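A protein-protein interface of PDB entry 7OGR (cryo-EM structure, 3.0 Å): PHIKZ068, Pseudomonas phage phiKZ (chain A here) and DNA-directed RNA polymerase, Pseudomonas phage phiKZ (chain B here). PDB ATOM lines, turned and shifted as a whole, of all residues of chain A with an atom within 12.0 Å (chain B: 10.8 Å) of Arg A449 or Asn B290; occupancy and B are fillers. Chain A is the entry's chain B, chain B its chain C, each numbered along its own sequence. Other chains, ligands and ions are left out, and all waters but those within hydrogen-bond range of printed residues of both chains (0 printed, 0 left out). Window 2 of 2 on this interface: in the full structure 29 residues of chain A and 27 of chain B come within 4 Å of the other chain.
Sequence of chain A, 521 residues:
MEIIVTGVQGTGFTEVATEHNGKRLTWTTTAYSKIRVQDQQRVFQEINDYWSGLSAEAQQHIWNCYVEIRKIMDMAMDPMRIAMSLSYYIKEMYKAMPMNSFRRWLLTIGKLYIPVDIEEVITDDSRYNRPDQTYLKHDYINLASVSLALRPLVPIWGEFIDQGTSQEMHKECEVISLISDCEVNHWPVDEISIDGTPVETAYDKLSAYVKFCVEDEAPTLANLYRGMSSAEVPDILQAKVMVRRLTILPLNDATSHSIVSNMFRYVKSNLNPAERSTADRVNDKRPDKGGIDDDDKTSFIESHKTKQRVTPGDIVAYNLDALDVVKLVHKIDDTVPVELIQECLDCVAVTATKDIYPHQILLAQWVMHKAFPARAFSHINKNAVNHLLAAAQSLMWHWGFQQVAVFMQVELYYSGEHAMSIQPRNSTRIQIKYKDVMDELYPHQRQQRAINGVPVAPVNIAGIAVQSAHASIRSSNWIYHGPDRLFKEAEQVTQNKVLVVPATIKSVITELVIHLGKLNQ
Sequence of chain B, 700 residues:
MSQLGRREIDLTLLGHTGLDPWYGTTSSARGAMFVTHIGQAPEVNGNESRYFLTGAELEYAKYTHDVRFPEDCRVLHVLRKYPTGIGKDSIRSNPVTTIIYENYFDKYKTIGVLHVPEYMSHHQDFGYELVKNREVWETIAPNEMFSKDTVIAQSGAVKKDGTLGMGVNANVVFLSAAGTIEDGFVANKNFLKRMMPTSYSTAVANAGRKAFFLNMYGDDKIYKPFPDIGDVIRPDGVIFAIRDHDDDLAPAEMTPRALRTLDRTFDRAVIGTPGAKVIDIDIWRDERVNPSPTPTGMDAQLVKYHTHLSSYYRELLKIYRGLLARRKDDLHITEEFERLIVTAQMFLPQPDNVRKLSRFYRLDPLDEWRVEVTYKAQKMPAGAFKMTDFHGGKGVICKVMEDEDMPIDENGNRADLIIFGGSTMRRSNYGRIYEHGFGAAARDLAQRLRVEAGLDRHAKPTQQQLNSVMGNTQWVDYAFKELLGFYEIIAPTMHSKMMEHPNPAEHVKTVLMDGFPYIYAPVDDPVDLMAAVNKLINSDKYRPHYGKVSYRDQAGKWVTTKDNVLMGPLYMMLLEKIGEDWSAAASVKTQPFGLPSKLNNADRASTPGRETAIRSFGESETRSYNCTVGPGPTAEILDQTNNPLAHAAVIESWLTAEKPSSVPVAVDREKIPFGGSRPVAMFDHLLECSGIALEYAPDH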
ATOM      1  N   GLN A 445      10.628 -16.885 -24.776  1.00  0.00           N
ATOM      2  CA  GLN A 445      12.077 -16.775 -24.819  1.00  0.00           C
ATOM      3  C   GLN A 445      12.612 -16.346 -23.459  1.00  0.00           C
ATOM      4  O   GLN A 445      11.876 -15.838 -22.609  1.00  0.00           O
ATOM      5  CB  GLN A 445      12.512 -15.778 -25.899  1.00  0.00           C
ATOM      6  CG  GLN A 445      12.390 -16.322 -27.311  1.00  0.00           C
ATOM      7  CD  GLN A 445      11.966 -15.267 -28.311  1.00  0.00           C
ATOM      8  OE1 GLN A 445      11.907 -14.080 -27.992  1.00  0.00           O
ATOM      9  NE2 GLN A 445      11.663 -15.697 -29.528  1.00  0.00           N
ATOM     10  N   ARG A 446      13.913 -16.548 -23.266  1.00  0.00           N
ATOM     11  CA  ARG A 446      14.559 -16.239 -21.996  1.00  0.00           C
ATOM     12  C   ARG A 446      14.928 -14.761 -21.947  1.00  0.00           C
ATOM     13  O   ARG A 446      15.608 -14.256 -22.848  1.00  0.00           O
ATOM     14  CB  ARG A 446      15.799 -17.110 -21.807  1.00  0.00           C
ATOM     15  CG  ARG A 446      16.643 -16.746 -20.595  1.00  0.00           C
ATOM     16  CD  ARG A 446      15.880 -16.965 -19.297  1.00  0.00           C
ATOM     17  NE  ARG A 446      15.233 -18.273 -19.248  1.00  0.00           N
ATOM     18  CZ  ARG A 446      15.827 -19.385 -18.829  1.00  0.00           C
ATOM     19  NH1 ARG A 446      17.089 -19.353 -18.422  1.00  0.00           N
ATOM     20  NH2 ARG A 446      15.160 -20.531 -18.815  1.00  0.00           N
ATOM     21  N   GLN A 447      14.463 -14.068 -20.907  1.00  0.00           N
ATOM     22  CA  GLN A 447      14.814 -12.667 -20.701  1.00  0.00           C
ATOM     23  C   GLN A 447      16.302 -12.523 -20.405  1.00  0.00           C
ATOM     24  O   GLN A 447      16.916 -13.393 -19.780  1.00  0.00           O
ATOM     25  CB  GLN A 447      13.989 -12.084 -19.553  1.00  0.00           C
ATOM     26  CG  GLN A 447      12.542 -11.779 -19.908  1.00  0.00           C
ATOM     27  CD  GLN A 447      12.377 -10.436 -20.586  1.00  0.00           C
ATOM     28  OE1 GLN A 447      12.173 -10.358 -21.797  1.00  0.00           O
ATOM     29  NE2 GLN A 447      12.463  -9.364 -19.805  1.00  0.00           N
ATOM     30  N   GLN A 448      16.884 -11.417 -20.861  1.00  0.00           N
ATOM     31  CA  GLN A 448      18.318 -11.193 -20.763  1.00  0.00           C
ATOM     32  C   GLN A 448      18.611  -9.917 -19.983  1.00  0.00           C
ATOM     33  O   GLN A 448      17.793  -8.994 -19.934  1.00  0.00           O
ATOM     34  CB  GLN A 448      18.959 -11.106 -22.151  1.00  0.00           C
ATOM     35  CG  GLN A 448      19.082 -12.444 -22.861  1.00  0.00           C
ATOM     36  CD  GLN A 448      20.232 -13.282 -22.329  1.00  0.00           C
ATOM     37  OE1 GLN A 448      20.046 -14.436 -21.947  1.00  0.00           O
ATOM     38  NE2 GLN A 448      21.423 -12.699 -22.295  1.00  0.00           N
ATOM     39  N   ARG A 449      19.793  -9.885 -19.374  1.00  0.00           N
ATOM     40  CA  ARG A 449      20.244  -8.748 -18.584  1.00  0.00           C
ATOM     41  C   ARG A 449      20.883  -7.704 -19.492  1.00  0.00           C
ATOM     42  O   ARG A 449      21.742  -8.033 -20.317  1.00  0.00           O
ATOM     43  CB  ARG A 449      21.237  -9.208 -17.515  1.00  0.00           C
ATOM     44  CG  ARG A 449      21.956  -8.088 -16.784  1.00  0.00           C
ATOM     45  CD  ARG A 449      23.196  -8.598 -16.058  1.00  0.00           C
ATOM     46  NE  ARG A 449      22.862  -9.408 -14.887  1.00  0.00           N
ATOM     47  CZ  ARG A 449      22.975 -10.732 -14.833  1.00  0.00           C
ATOM     48  NH1 ARG A 449      23.412 -11.405 -15.889  1.00  0.00           N
ATOM     49  NH2 ARG A 449      22.648 -11.383 -13.725  1.00  0.00           N
ATOM     50  N   ALA A 450      20.459  -6.451 -19.340  1.00  0.00           N
ATOM     51  CA  ALA A 450      21.009  -5.363 -20.138  1.00  0.00           C
ATOM     52  C   ALA A 450      22.429  -5.034 -19.697  1.00  0.00           C
ATOM     53  O   ALA A 450      22.761  -5.101 -18.510  1.00  0.00           O
ATOM     54  CB  ALA A 450      20.122  -4.125 -20.026  1.00  0.00           C
ATOM     55  N   ILE A 451      23.271  -4.672 -20.663  1.00  0.00           N
ATOM     56  CA  ILE A 451      24.683  -4.386 -20.421  1.00  0.00           C
ATOM     57  C   ILE A 451      24.933  -2.952 -20.871  1.00  0.00           C
ATOM     58  O   ILE A 451      25.020  -2.680 -22.077  1.00  0.00           O
ATOM     59  CB  ILE A 451      25.611  -5.367 -21.148  1.00  0.00           C
ATOM     60  CG1 ILE A 451      25.334  -6.805 -20.691  1.00  0.00           C
ATOM     61  CG2 ILE A 451      27.076  -4.987 -20.910  1.00  0.00           C
ATOM     62  CD1 ILE A 451      26.379  -7.821 -21.131  1.00  0.00           C
ATOM     63  N   ASN A 452      25.043  -2.040 -19.899  1.00  0.00           N
ATOM     64  CA  ASN A 452      25.379  -0.622 -20.082  1.00  0.00           C
ATOM     65  C   ASN A 452      24.380   0.081 -21.009  1.00  0.00           C
ATOM     66  O   ASN A 452      24.724   0.613 -22.066  1.00  0.00           O
ATOM     67  CB  ASN A 452      26.820  -0.458 -20.585  1.00  0.00           C
ATOM     68  CG  ASN A 452      27.847  -0.821 -19.532  1.00  0.00           C
ATOM     69  OD1 ASN A 452      27.701  -0.477 -18.359  1.00  0.00           O
ATOM     70  ND2 ASN A 452      28.896  -1.524 -19.946  1.00  0.00           N
ATOM     71  N   GLY A 453      23.126   0.079 -20.556  1.00  0.00           N
ATOM     72  CA  GLY A 453      22.035   0.796 -21.194  1.00  0.00           C
ATOM     73  C   GLY A 453      21.702   0.450 -22.633  1.00  0.00           C
ATOM     74  O   GLY A 453      21.636   1.341 -23.486  1.00  0.00           O
ATOM     75  N   VAL A 454      21.484  -0.830 -22.916  1.00  0.00           N
ATOM     76  CA  VAL A 454      20.948  -1.259 -24.207  1.00  0.00           C
ATOM     77  C   VAL A 454      20.088  -2.501 -23.981  1.00  0.00           C
ATOM     78  O   VAL A 454      20.507  -3.436 -23.280  1.00  0.00           O
ATOM     79  CB  VAL A 454      22.067  -1.464 -25.253  1.00  0.00           C
ATOM     80  CG1 VAL A 454      23.137  -2.459 -24.798  1.00  0.00           C
ATOM     81  CG2 VAL A 454      21.477  -1.888 -26.594  1.00  0.00           C
ATOM     82  N   PRO A 455      18.844  -2.519 -24.466  1.00  0.00           N
ATOM     83  CA  PRO A 455      17.994  -3.705 -24.273  1.00  0.00           C
ATOM     84  C   PRO A 455      18.463  -4.862 -25.145  1.00  0.00           C
ATOM     85  O   PRO A 455      18.449  -4.778 -26.376  1.00  0.00           O
ATOM     86  CB  PRO A 455      16.597  -3.214 -24.674  1.00  0.00           C
ATOM     87  CG  PRO A 455      16.837  -2.033 -25.550  1.00  0.00           C
ATOM     88  CD  PRO A 455      18.099  -1.390 -25.052  1.00  0.00           C
ATOM     89  N   VAL A 456      18.890  -5.939 -24.499  1.00  0.00           N
ATOM     90  CA  VAL A 456      19.322  -7.137 -25.204  1.00  0.00           C
ATOM     91  C   VAL A 456      18.096  -7.899 -25.683  1.00  0.00           C
ATOM     92  O   VAL A 456      17.090  -8.001 -24.968  1.00  0.00           O
ATOM     93  CB  VAL A 456      20.210  -8.008 -24.296  1.00  0.00           C
ATOM     94  CG1 VAL A 456      20.983  -9.032 -25.118  1.00  0.00           C
ATOM     95  CG2 VAL A 456      21.163  -7.138 -23.501  1.00  0.00           C
ATOM     96  N   ALA A 457      18.169  -8.416 -26.907  1.00  0.00           N
ATOM     97  CA  ALA A 457      17.098  -9.248 -27.432  1.00  0.00           C
ATOM     98  C   ALA A 457      17.052 -10.574 -26.674  1.00  0.00           C
ATOM     99  O   ALA A 457      18.101 -11.100 -26.285  1.00  0.00           O
ATOM    100  CB  ALA A 457      17.303  -9.500 -28.926  1.00  0.00           C
ATOM    101  N   PRO A 458      15.862 -11.121 -26.424  1.00  0.00           N
ATOM    102  CA  PRO A 458      15.774 -12.363 -25.648  1.00  0.00           C
ATOM    103  C   PRO A 458      16.296 -13.565 -26.420  1.00  0.00           C
ATOM    104  O   PRO A 458      16.131 -13.680 -27.637  1.00  0.00           O
ATOM    105  CB  PRO A 458      14.274 -12.501 -25.361  1.00  0.00           C
ATOM    106  CG  PRO A 458      13.602 -11.673 -26.395  1.00  0.00           C
ATOM    107  CD  PRO A 458      14.534 -10.546 -26.703  1.00  0.00           C
ATOM    108  N   VAL A 459      16.934 -14.467 -25.683  1.00  0.00           N
ATOM    109  CA  VAL A 459      17.537 -15.667 -26.248  1.00  0.00           C
ATOM    110  C   VAL A 459      16.456 -16.733 -26.368  1.00  0.00           C
ATOM    111  O   VAL A 459      15.669 -16.935 -25.435  1.00  0.00           O
ATOM    112  CB  VAL A 459      18.711 -16.146 -25.372  1.00  0.00           C
ATOM    113  CG1 VAL A 459      19.212 -17.521 -25.793  1.00  0.00           C
ATOM    114  CG2 VAL A 459      19.845 -15.131 -25.413  1.00  0.00           C
ATOM    115  N   ASN A 460      16.393 -17.388 -27.529  1.00  0.00           N
ATOM    116  CA  ASN A 460      15.417 -18.448 -27.748  1.00  0.00           C
ATOM    117  C   ASN A 460      15.712 -19.645 -26.854  1.00  0.00           C
ATOM    118  O   ASN A 460      16.864 -20.055 -26.689  1.00  0.00           O
ATOM    119  CB  ASN A 460      15.416 -18.878 -29.215  1.00  0.00           C
ATOM    120  CG  ASN A 460      14.079 -19.448 -29.655  1.00  0.00           C
ATOM    121  OD1 ASN A 460      13.265 -19.861 -28.832  1.00  0.00           O
ATOM    122  ND2 ASN A 460      13.846 -19.464 -30.961  1.00  0.00           N
ATOM    123  N   ILE A 464      19.356 -23.210 -26.802  1.00  0.00           N
ATOM    124  CA  ILE A 464      20.217 -23.729 -25.745  1.00  0.00           C
ATOM    125  C   ILE A 464      20.123 -25.249 -25.688  1.00  0.00           C
ATOM    126  O   ILE A 464      21.124 -25.935 -25.444  1.00  0.00           O
ATOM    127  CB  ILE A 464      19.837 -23.074 -24.401  1.00  0.00           C
ATOM    128  CG1 ILE A 464      19.906 -21.551 -24.520  1.00  0.00           C
ATOM    129  CG2 ILE A 464      20.760 -23.529 -23.281  1.00  0.00           C
ATOM    130  CD1 ILE A 464      19.292 -20.821 -23.346  1.00  0.00           C
ATOM    131  N   ARG B 285       4.197  -8.654  -6.759  1.00  0.00           N
ATOM    132  CA  ARG B 285       5.308  -8.806  -7.690  1.00  0.00           C
ATOM    133  C   ARG B 285       6.572  -8.198  -7.102  1.00  0.00           C
ATOM    134  O   ARG B 285       6.561  -7.048  -6.654  1.00  0.00           O
ATOM    135  CB  ARG B 285       4.991  -8.149  -9.038  1.00  0.00           C
ATOM    136  CG  ARG B 285       6.146  -8.158 -10.027  1.00  0.00           C
ATOM    137  CD  ARG B 285       5.891  -7.211 -11.186  1.00  0.00           C
ATOM    138  NE  ARG B 285       6.704  -7.546 -12.352  1.00  0.00           N
ATOM    139  CZ  ARG B 285       6.452  -7.119 -13.585  1.00  0.00           C
ATOM    140  NH1 ARG B 285       7.245  -7.473 -14.586  1.00  0.00           N
ATOM    141  NH2 ARG B 285       5.406  -6.339 -13.816  1.00  0.00           N
ATOM    142  N   ASP B 286       7.655  -8.975  -7.107  1.00  0.00           N
ATOM    143  CA  ASP B 286       8.984  -8.476  -6.754  1.00  0.00           C
ATOM    144  C   ASP B 286       9.646  -8.011  -8.044  1.00  0.00           C
ATOM    145  O   ASP B 286      10.280  -8.786  -8.760  1.00  0.00           O
ATOM    146  CB  ASP B 286       9.798  -9.554  -6.049  1.00  0.00           C
ATOM    147  CG  ASP B 286      11.219  -9.113  -5.751  1.00  0.00           C
ATOM    148  OD1 ASP B 286      11.421  -7.926  -5.418  1.00  0.00           O
ATOM    149  OD2 ASP B 286      12.135  -9.956  -5.852  1.00  0.00           O
ATOM    150  N   GLU B 287       9.493  -6.721  -8.346  1.00  0.00           N
ATOM    151  CA  GLU B 287       9.961  -6.146  -9.602  1.00  0.00           C
ATOM    152  C   GLU B 287      11.334  -5.494  -9.474  1.00  0.00           C
ATOM    153  O   GLU B 287      11.638  -4.544 -10.203  1.00  0.00           O
ATOM    154  CB  GLU B 287       8.945  -5.135 -10.131  1.00  0.00           C
ATOM    155  CG  GLU B 287       8.518  -4.087  -9.118  1.00  0.00           C
ATOM    156  CD  GLU B 287       7.373  -3.229  -9.616  1.00  0.00           C
ATOM    157  OE1 GLU B 287       6.211  -3.679  -9.533  1.00  0.00           O
ATOM    158  OE2 GLU B 287       7.635  -2.105 -10.093  1.00  0.00           O
ATOM    159  N   ARG B 288      12.178  -5.987  -8.567  1.00  0.00           N
ATOM    160  CA  ARG B 288      13.526  -5.459  -8.407  1.00  0.00           C
ATOM    161  C   ARG B 288      14.594  -6.420  -8.916  1.00  0.00           C
ATOM    162  O   ARG B 288      15.783  -6.209  -8.660  1.00  0.00           O
ATOM    163  CB  ARG B 288      13.796  -5.095  -6.948  1.00  0.00           C
ATOM    164  CG  ARG B 288      13.258  -3.735  -6.549  1.00  0.00           C
ATOM    165  CD  ARG B 288      14.215  -2.630  -6.972  1.00  0.00           C
ATOM    166  NE  ARG B 288      15.362  -2.512  -6.078  1.00  0.00           N
ATOM    167  CZ  ARG B 288      15.424  -1.674  -5.048  1.00  0.00           C
ATOM    168  NH1 ARG B 288      16.510  -1.634  -4.289  1.00  0.00           N
ATOM    169  NH2 ARG B 288      14.401  -0.875  -4.779  1.00  0.00           N
ATOM    170  N   VAL B 289      14.197  -7.471  -9.625  1.00  0.00           N
ATOM    171  CA  VAL B 289      15.148  -8.320 -10.333  1.00  0.00           C
ATOM    172  C   VAL B 289      15.309  -7.793 -11.757  1.00  0.00           C
ATOM    173  O   VAL B 289      14.323  -7.567 -12.468  1.00  0.00           O
ATOM    174  CB  VAL B 289      14.710  -9.798 -10.300  1.00  0.00           C
ATOM    175  CG1 VAL B 289      14.935 -10.368  -8.913  1.00  0.00           C
ATOM    176  CG2 VAL B 289      13.232  -9.962 -10.646  1.00  0.00           C
ATOM    177  N   ASN B 290      16.552  -7.535 -12.154  1.00  0.00           N
ATOM    178  CA  ASN B 290      16.767  -7.000 -13.495  1.00  0.00           C
ATOM    179  C   ASN B 290      16.823  -8.086 -14.580  1.00  0.00           C
ATOM    180  O   ASN B 290      16.517  -7.766 -15.736  1.00  0.00           O
ATOM    181  CB  ASN B 290      17.974  -6.032 -13.506  1.00  0.00           C
ATOM    182  CG  ASN B 290      19.336  -6.709 -13.474  1.00  0.00           C
ATOM    183  OD1 ASN B 290      19.772  -7.322 -14.446  1.00  0.00           O
ATOM    184  ND2 ASN B 290      20.016  -6.598 -12.340  1.00  0.00           N
ATOM    185  N   PRO B 291      17.200  -9.387 -14.308  1.00  0.00           N
ATOM    186  CA  PRO B 291      16.707 -10.429 -15.222  1.00  0.00           C
ATOM    187  C   PRO B 291      15.427 -11.082 -14.717  1.00  0.00           C
ATOM    188  O   PRO B 291      15.323 -11.447 -13.542  1.00  0.00           O
ATOM    189  CB  PRO B 291      17.871 -11.424 -15.292  1.00  0.00           C
ATOM    190  CG  PRO B 291      18.577 -11.283 -14.017  1.00  0.00           C
ATOM    191  CD  PRO B 291      18.230  -9.956 -13.405  1.00  0.00           C
ATOM    192  N   SER B 292      14.443 -11.236 -15.594  1.00  0.00           N
ATOM    193  CA  SER B 292      13.216 -11.899 -15.159  1.00  0.00           C
ATOM    194  C   SER B 292      13.277 -13.384 -15.495  1.00  0.00           C
ATOM    195  O   SER B 292      13.480 -13.738 -16.662  1.00  0.00           O
ATOM    196  CB  SER B 292      11.996 -11.272 -15.818  1.00  0.00           C
ATOM    197  OG  SER B 292      10.806 -11.659 -15.153  1.00  0.00           O
ATOM    198  N   PRO B 293      13.111 -14.279 -14.514  1.00  0.00           N
ATOM    199  CA  PRO B 293      13.080 -15.715 -14.827  1.00  0.00           C
ATOM    200  C   PRO B 293      11.788 -16.170 -15.485  1.00  0.00           C
ATOM    201  O   PRO B 293      11.753 -17.281 -16.035  1.00  0.00           O
ATOM    202  CB  PRO B 293      13.261 -16.380 -13.455  1.00  0.00           C
ATOM    203  CG  PRO B 293      12.802 -15.369 -12.473  1.00  0.00           C
ATOM    204  CD  PRO B 293      13.066 -14.017 -13.067  1.00  0.00           C
ATOM    205  N   THR B 294      10.741 -15.359 -15.449  1.00  0.00           N
ATOM    206  CA  THR B 294       9.539 -15.657 -16.212  1.00  0.00           C
ATOM    207  C   THR B 294       9.808 -15.390 -17.689  1.00  0.00           C
ATOM    208  O   THR B 294      10.265 -14.294 -18.041  1.00  0.00           O
ATOM    209  CB  THR B 294       8.369 -14.805 -15.722  1.00  0.00           C
ATOM    210  OG1 THR B 294       8.270 -14.904 -14.295  1.00  0.00           O
ATOM    211  CG2 THR B 294       7.065 -15.273 -16.347  1.00  0.00           C
ATOM    212  N   THR B 296       9.096 -14.810 -21.869  1.00  0.00           N
ATOM    213  CA  THR B 296       8.341 -13.777 -22.563  1.00  0.00           C
ATOM    214  C   THR B 296       6.958 -14.298 -22.964  1.00  0.00           C
ATOM    215  O   THR B 296       6.796 -15.440 -23.402  1.00  0.00           O
ATOM    216  CB  THR B 296       9.132 -13.309 -23.794  1.00  0.00           C
ATOM    217  OG1 THR B 296      10.424 -12.845 -23.382  1.00  0.00           O
ATOM    218  CG2 THR B 296       8.435 -12.172 -24.540  1.00  0.00           C
ATOM    219  N   ASP B 352      16.005   3.065  -5.768  1.00  0.00           N
ATOM    220  CA  ASP B 352      17.221   2.257  -5.791  1.00  0.00           C
ATOM    221  C   ASP B 352      18.302   2.778  -4.838  1.00  0.00           C
ATOM    222  O   ASP B 352      19.423   2.260  -4.849  1.00  0.00           O
ATOM    223  CB  ASP B 352      17.769   2.192  -7.221  1.00  0.00           C
ATOM    224  CG  ASP B 352      18.387   0.841  -7.561  1.00  0.00           C
ATOM    225  OD1 ASP B 352      18.367   0.470  -8.753  1.00  0.00           O
ATOM    226  OD2 ASP B 352      18.865   0.132  -6.652  1.00  0.00           O
ATOM    227  N   LYS B 356      16.040  -3.465  -1.294  1.00  0.00           N
ATOM    228  CA  LYS B 356      14.693  -3.883  -1.644  1.00  0.00           C
ATOM    229  C   LYS B 356      14.095  -4.742  -0.533  1.00  0.00           C
ATOM    230  O   LYS B 356      14.801  -5.301   0.308  1.00  0.00           O
ATOM    231  CB  LYS B 356      14.692  -4.657  -2.964  1.00  0.00           C
ATOM    232  CG  LYS B 356      15.589  -5.884  -2.973  1.00  0.00           C
ATOM    233  CD  LYS B 356      14.999  -6.982  -3.846  1.00  0.00           C
ATOM    234  CE  LYS B 356      15.914  -8.195  -3.916  1.00  0.00           C
ATOM    235  NZ  LYS B 356      16.130  -8.817  -2.580  1.00  0.00           N
ATOM    236  N   GLU B 368       8.891 -13.501  -6.585  1.00  0.00           N
ATOM    237  CA  GLU B 368       8.621 -12.697  -7.782  1.00  0.00           C
ATOM    238  C   GLU B 368       7.155 -12.662  -8.216  1.00  0.00           C
ATOM    239  O   GLU B 368       6.764 -11.770  -8.975  1.00  0.00           O
ATOM    240  CB  GLU B 368       9.496 -13.179  -8.951  1.00  0.00           C
ATOM    241  CG  GLU B 368       9.811 -12.122 -10.003  1.00  0.00           C
ATOM    242  CD  GLU B 368      10.092 -12.726 -11.362  1.00  0.00           C
ATOM    243  OE1 GLU B 368       9.942 -13.958 -11.505  1.00  0.00           O
ATOM    244  OE2 GLU B 368      10.460 -11.973 -12.287  1.00  0.00           O
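O of Gln A445 is in hydrogen-bond range of N of Thr B296 (3.1 Å). OG1 of Thr B296 lies within hydrogen-bond range of OE1 of Gln A447 (3.4 Å).
The side-chain hydroxyl of Ser B292 is in hydrogen-bond range of the side-chain carboxylate of Glu B368 (2.9 Å). The side-chain carboxylate (OE1) of Glu B368 is in hydrogen-bond range of the side-chain hydroxyl (OG1) of Thr B294 (3.4 Å).
Gln A447 touches Ser B292 (CB to O, 3.4 Å). Gln A447 touches Thr B294. CG of Arg A449 touches OD1 of Asn B290 (3.3 Å).
Printed residues of chain B within 4 Å of Gln A445: Thr B296 (3.1 Å). Printed residues of chain B within 4 Å of Gln A447: Ser B292, Thr B294 and Thr B296. No residue of chain B comes within 4 Å of Gln A448. Of chain B, only Asn B290 (3.3 Å) comes within 4 Å of Arg A449. No residue of chain B comes within 4 Å of Ala A450. No residue of chain B comes within 4 Å of Ile A451. Asp B286 touches none of the printed residues of chain A. No residue of chain A comes within 4 Å of Val B289. Of the printed residues of chain A, Asn B290 touches Arg A449. Of chain A, only Gln A447 (3.4 Å) comes within 4 Å of Ser B292. Of the printed residues of chain A, Thr B294 touches Gln A447 (3.9 Å). Of the printed residues of chain A, Thr B296 touches Gln A445 and Gln A447. The nearest printed residue of chain A that does not touch Thr B296 is Pro A458 (4.3 Å).
Of the 17 printed residues of chain A, 3 touch a printed residue of chain B. Printed residues of chain A that touch a printed residue of chain B: Gln A445, Gln A447 and Arg A449. Among the printed residues, no Asp or Glu carboxylate lies within 4 Å of a Lys or Arg side-chain nitrogen of the other chain.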
